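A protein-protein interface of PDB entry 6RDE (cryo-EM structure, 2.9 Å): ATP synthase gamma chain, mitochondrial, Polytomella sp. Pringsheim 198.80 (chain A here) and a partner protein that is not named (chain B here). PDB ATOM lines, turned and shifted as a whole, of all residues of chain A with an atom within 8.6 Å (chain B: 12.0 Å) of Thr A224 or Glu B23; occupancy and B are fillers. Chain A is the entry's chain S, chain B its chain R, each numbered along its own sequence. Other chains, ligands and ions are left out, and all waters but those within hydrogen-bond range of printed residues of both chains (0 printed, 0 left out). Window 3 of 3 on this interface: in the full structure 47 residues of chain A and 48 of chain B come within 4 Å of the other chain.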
ATOM      1  N   LEU A 216     -19.730  -4.580 -19.865  1.00  0.00           N
ATOM      2  CA  LEU A 216     -18.410  -4.314 -19.301  1.00  0.00           C
ATOM      3  C   LEU A 216     -17.253  -4.923 -20.076  1.00  0.00           C
ATOM      4  O   LEU A 216     -16.123  -4.452 -19.914  1.00  0.00           O
ATOM      5  CB  LEU A 216     -18.338  -4.804 -17.849  1.00  0.00           C
ATOM      6  CG  LEU A 216     -17.394  -4.004 -16.948  1.00  0.00           C
ATOM      7  CD1 LEU A 216     -18.031  -2.678 -16.554  1.00  0.00           C
ATOM      8  CD2 LEU A 216     -16.963  -4.792 -15.736  1.00  0.00           C
ATOM      9  N   LYS A 218     -16.722  -4.997 -23.438  1.00  0.00           N
ATOM     10  CA  LYS A 218     -16.314  -4.029 -24.448  1.00  0.00           C
ATOM     11  C   LYS A 218     -15.648  -2.801 -23.854  1.00  0.00           C
ATOM     12  O   LYS A 218     -14.830  -2.171 -24.531  1.00  0.00           O
ATOM     13  CB  LYS A 218     -17.514  -3.569 -25.266  1.00  0.00           C
ATOM     14  CG  LYS A 218     -18.084  -4.605 -26.186  1.00  0.00           C
ATOM     15  CD  LYS A 218     -19.297  -4.052 -26.907  1.00  0.00           C
ATOM     16  CE  LYS A 218     -18.900  -3.061 -27.976  1.00  0.00           C
ATOM     17  NZ  LYS A 218     -18.233  -3.756 -29.104  1.00  0.00           N
ATOM     18  N   GLN A 219     -15.958  -2.464 -22.603  1.00  0.00           N
ATOM     19  CA  GLN A 219     -15.436  -1.238 -22.020  1.00  0.00           C
ATOM     20  C   GLN A 219     -13.998  -1.396 -21.558  1.00  0.00           C
ATOM     21  O   GLN A 219     -13.225  -0.437 -21.626  1.00  0.00           O
ATOM     22  CB  GLN A 219     -16.338  -0.799 -20.874  1.00  0.00           C
ATOM     23  CG  GLN A 219     -17.707  -0.382 -21.361  1.00  0.00           C
ATOM     24  CD  GLN A 219     -18.560   0.222 -20.280  1.00  0.00           C
ATOM     25  OE1 GLN A 219     -18.104   0.433 -19.159  1.00  0.00           O
ATOM     26  NE2 GLN A 219     -19.816   0.497 -20.607  1.00  0.00           N
ATOM     27  N   LEU A 220     -13.617  -2.587 -21.096  1.00  0.00           N
ATOM     28  CA  LEU A 220     -12.229  -2.820 -20.705  1.00  0.00           C
ATOM     29  C   LEU A 220     -11.309  -2.978 -21.904  1.00  0.00           C
ATOM     30  O   LEU A 220     -10.085  -2.939 -21.742  1.00  0.00           O
ATOM     31  CB  LEU A 220     -12.109  -4.065 -19.824  1.00  0.00           C
ATOM     32  CG  LEU A 220     -12.157  -3.934 -18.301  1.00  0.00           C
ATOM     33  CD1 LEU A 220     -10.940  -3.167 -17.818  1.00  0.00           C
ATOM     34  CD2 LEU A 220     -13.448  -3.311 -17.794  1.00  0.00           C
ATOM     35  N   GLU A 221     -11.861  -3.189 -23.092  1.00  0.00           N
ATOM     36  CA  GLU A 221     -11.053  -3.362 -24.286  1.00  0.00           C
ATOM     37  C   GLU A 221     -10.741  -2.048 -24.978  1.00  0.00           C
ATOM     38  O   GLU A 221      -9.974  -2.040 -25.946  1.00  0.00           O
ATOM     39  CB  GLU A 221     -11.750  -4.307 -25.264  1.00  0.00           C
ATOM     40  CG  GLU A 221     -11.939  -5.693 -24.722  1.00  0.00           C
ATOM     41  CD  GLU A 221     -10.630  -6.376 -24.451  1.00  0.00           C
ATOM     42  OE1 GLU A 221      -9.713  -6.258 -25.285  1.00  0.00           O
ATOM     43  OE2 GLU A 221     -10.510  -7.023 -23.397  1.00  0.00           O
ATOM     44  N   ASP A 222     -11.293  -0.938 -24.491  1.00  0.00           N
ATOM     45  CA  ASP A 222     -11.091   0.368 -25.113  1.00  0.00           C
ATOM     46  C   ASP A 222      -9.753   0.954 -24.664  1.00  0.00           C
ATOM     47  O   ASP A 222      -9.670   1.930 -23.921  1.00  0.00           O
ATOM     48  CB  ASP A 222     -12.246   1.300 -24.782  1.00  0.00           C
ATOM     49  CG  ASP A 222     -13.489   0.993 -25.587  1.00  0.00           C
ATOM     50  OD1 ASP A 222     -14.600   1.297 -25.110  1.00  0.00           O
ATOM     51  OD2 ASP A 222     -13.356   0.446 -26.702  1.00  0.00           O
ATOM     52  N   VAL A 223      -8.682   0.342 -25.149  1.00  0.00           N
ATOM     53  CA  VAL A 223      -7.327   0.795 -24.870  1.00  0.00           C
ATOM     54  C   VAL A 223      -6.804   1.418 -26.156  1.00  0.00           C
ATOM     55  O   VAL A 223      -6.567   0.703 -27.138  1.00  0.00           O
ATOM     56  CB  VAL A 223      -6.422  -0.345 -24.385  1.00  0.00           C
ATOM     57  CG1 VAL A 223      -5.035   0.182 -24.061  1.00  0.00           C
ATOM     58  CG2 VAL A 223      -7.041  -1.024 -23.176  1.00  0.00           C
ATOM     59  N   THR A 224      -6.630   2.748 -26.132  1.00  0.00           N
ATOM     60  CA  THR A 224      -6.318   3.654 -27.259  1.00  0.00           C
ATOM     61  C   THR A 224      -7.096   3.273 -28.525  1.00  0.00           C
ATOM     62  O   THR A 224      -6.538   2.948 -29.571  1.00  0.00           O
ATOM     63  CB  THR A 224      -4.793   3.828 -27.516  1.00  0.00           C
ATOM     64  OG1 THR A 224      -4.593   4.648 -28.675  1.00  0.00           O
ATOM     65  CG2 THR A 224      -3.962   2.529 -27.672  1.00  0.00           C
ATOM     66  N   GLY A 225      -8.421   3.337 -28.404  1.00  0.00           N
ATOM     67  CA  GLY A 225      -9.333   2.862 -29.430  1.00  0.00           C
ATOM     68  C   GLY A 225     -10.083   1.626 -28.981  1.00  0.00           C
ATOM     69  O   GLY A 225     -10.964   1.733 -28.123  1.00  0.00           O
ATOM     70  N   ASN A 226      -9.754   0.462 -29.543  1.00  0.00           N
ATOM     71  CA  ASN A 226     -10.265  -0.811 -29.045  1.00  0.00           C
ATOM     72  C   ASN A 226      -9.350  -1.938 -29.503  1.00  0.00           C
ATOM     73  O   ASN A 226      -8.751  -1.875 -30.579  1.00  0.00           O
ATOM     74  CB  ASN A 226     -11.698  -1.085 -29.505  1.00  0.00           C
ATOM     75  CG  ASN A 226     -12.423  -2.046 -28.595  1.00  0.00           C
ATOM     76  OD1 ASN A 226     -11.957  -3.156 -28.350  1.00  0.00           O
ATOM     77  ND2 ASN A 226     -13.567  -1.621 -28.075  1.00  0.00           N
ATOM     78  N   SER A 227      -9.252  -2.968 -28.667  1.00  0.00           N
ATOM     79  CA  SER A 227      -8.451  -4.144 -28.968  1.00  0.00           C
ATOM     80  C   SER A 227      -9.231  -5.203 -29.714  1.00  0.00           C
ATOM     81  O   SER A 227      -8.634  -6.156 -30.220  1.00  0.00           O
ATOM     82  CB  SER A 227      -7.895  -4.758 -27.687  1.00  0.00           C
ATOM     83  OG  SER A 227      -7.173  -5.935 -27.983  1.00  0.00           O
ATOM     84  N   ASP A 229     -11.344  -4.512 -32.334  1.00  0.00           N
ATOM     85  CA  ASP A 229     -11.576  -4.109 -33.713  1.00  0.00           C
ATOM     86  C   ASP A 229     -10.594  -4.728 -34.691  1.00  0.00           C
ATOM     87  O   ASP A 229     -10.786  -4.584 -35.902  1.00  0.00           O
ATOM     88  CB  ASP A 229     -11.512  -2.592 -33.836  1.00  0.00           C
ATOM     89  CG  ASP A 229     -12.458  -1.902 -32.900  1.00  0.00           C
ATOM     90  OD1 ASP A 229     -13.367  -2.575 -32.381  1.00  0.00           O
ATOM     91  OD2 ASP A 229     -12.295  -0.689 -32.686  1.00  0.00           O
ATOM     92  N   GLU B  23     -11.481   6.002 -21.687  1.00  0.00           N
ATOM     93  CA  GLU B  23     -11.748   4.722 -22.328  1.00  0.00           C
ATOM     94  C   GLU B  23     -10.974   3.588 -21.662  1.00  0.00           C
ATOM     95  O   GLU B  23     -11.448   2.450 -21.607  1.00  0.00           O
ATOM     96  CB  GLU B  23     -11.415   4.791 -23.821  1.00  0.00           C
ATOM     97  CG  GLU B  23     -10.037   5.340 -24.157  1.00  0.00           C
ATOM     98  CD  GLU B  23      -9.737   5.273 -25.641  1.00  0.00           C
ATOM     99  OE1 GLU B  23     -10.594   4.770 -26.396  1.00  0.00           O
ATOM    100  OE2 GLU B  23      -8.651   5.727 -26.053  1.00  0.00           O
ATOM    101  N   ALA B  24      -9.784   3.900 -21.157  1.00  0.00           N
ATOM    102  CA  ALA B  24      -8.903   2.933 -20.510  1.00  0.00           C
ATOM    103  C   ALA B  24      -8.626   3.362 -19.078  1.00  0.00           C
ATOM    104  O   ALA B  24      -7.485   3.384 -18.611  1.00  0.00           O
ATOM    105  CB  ALA B  24      -7.603   2.765 -21.293  1.00  0.00           C
ATOM    106  N   ALA B  25      -9.695   3.720 -18.364  1.00  0.00           N
ATOM    107  CA  ALA B  25      -9.588   4.342 -17.051  1.00  0.00           C
ATOM    108  C   ALA B  25      -9.429   3.347 -15.907  1.00  0.00           C
ATOM    109  O   ALA B  25      -9.452   3.769 -14.745  1.00  0.00           O
ATOM    110  CB  ALA B  25     -10.812   5.224 -16.793  1.00  0.00           C
ATOM    111  N   ALA B  26      -9.294   2.047 -16.188  1.00  0.00           N
ATOM    112  CA  ALA B  26      -9.055   1.035 -15.159  1.00  0.00           C
ATOM    113  C   ALA B  26      -8.206  -0.095 -15.733  1.00  0.00           C
ATOM    114  O   ALA B  26      -8.744  -1.109 -16.199  1.00  0.00           O
ATOM    115  CB  ALA B  26     -10.367   0.498 -14.594  1.00  0.00           C
ATOM    116  N   PRO B  27      -6.881   0.038 -15.709  1.00  0.00           N
ATOM    117  CA  PRO B  27      -6.022  -1.051 -16.194  1.00  0.00           C
ATOM    118  C   PRO B  27      -5.972  -2.231 -15.236  1.00  0.00           C
ATOM    119  O   PRO B  27      -5.124  -2.283 -14.339  1.00  0.00           O
ATOM    120  CB  PRO B  27      -4.647  -0.384 -16.332  1.00  0.00           C
ATOM    121  CG  PRO B  27      -4.910   1.086 -16.278  1.00  0.00           C
ATOM    122  CD  PRO B  27      -6.101   1.246 -15.403  1.00  0.00           C
ATOM    123  N   ALA B  28      -6.888  -3.177 -15.415  1.00  0.00           N
ATOM    124  CA  ALA B  28      -6.927  -4.397 -14.625  1.00  0.00           C
ATOM    125  C   ALA B  28      -5.944  -5.414 -15.197  1.00  0.00           C
ATOM    126  O   ALA B  28      -5.287  -5.174 -16.213  1.00  0.00           O
ATOM    127  CB  ALA B  28      -8.341  -4.962 -14.587  1.00  0.00           C
ATOM    128  N   VAL B  60      -1.752 -10.981 -29.144  1.00  0.00           N
ATOM    129  CA  VAL B  60      -1.284  -9.745 -29.762  1.00  0.00           C
ATOM    130  C   VAL B  60       0.175  -9.874 -30.193  1.00  0.00           C
ATOM    131  O   VAL B  60       0.586  -9.298 -31.208  1.00  0.00           O
ATOM    132  CB  VAL B  60      -1.514  -8.563 -28.800  1.00  0.00           C
ATOM    133  CG1 VAL B  60      -1.201  -7.240 -29.467  1.00  0.00           C
ATOM    134  CG2 VAL B  60      -2.949  -8.565 -28.300  1.00  0.00           C
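O of Glu B23 sits close to O of Gln A219 (3.4 Å).
N of Ala B24 lies within hydrogen-bond range of O of Asp A222 (3.4 Å).
OE1 of Glu B23 sits at hydrogen-bond distance from N of Gly A225, 3.3 Å away.
The backbone carbonyl oxygen of Asp A222 sits close to the backbone carbonyl oxygen of Glu B23 (3.0 Å).
ND2 of Asn A226 sits at hydrogen-bond distance from OD2 of Asp A222 (2.5 Å).
Among the printed residues, merely in contact across the chains: Leu A220 with Ala B26 (3.4 Å) and Thr A224 with Glu B23 (3.3 Å).
Printed residues of chain B within 4 Å of Gln A219: Glu B23 (3.4 Å).
Of chain B, only Ala B26 comes within 4 Å of Leu A220.
Asp A222 touches just these residues of chain B: Glu B23 and Ala B24.
No residue of chain B comes within 4 Å of Val A223.
Thr A224 touches just one residue of chain B: Glu B23 (3.3 Å).
Gly A225 touches one residue of chain B.
Of chain A, only Gln A219, Asp A222, Thr A224 and Gly A225 come within 4 Å of Glu B23.
Of the printed residues of chain A, Ala B26 touches Leu A220.
The nearest residue of chain A that does not touch Glu B23 is Val A223 (4.7 Å).
The nearest printed residue of chain B that does not touch Gln A219 is Ala B24 (5.6 Å).
Of the 7 printed residues of chain B, 3 touch a printed residue of chain A.
Along chain B the printed residues that touch a printed residue of chain A span positions 23 to 26.
Of the 12 printed residues of chain A, 5 touch a printed residue of chain B.
Hydrophobic or aromatic side chains of chain A that line the printed part of chain B: Leu A220.
Among the printed residues, 6 pairs touch across the chains.
Among the printed residues, no Asp or Glu carboxylate lies within 4 Å of a Lys or Arg side-chain nitrogen of the other chain.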
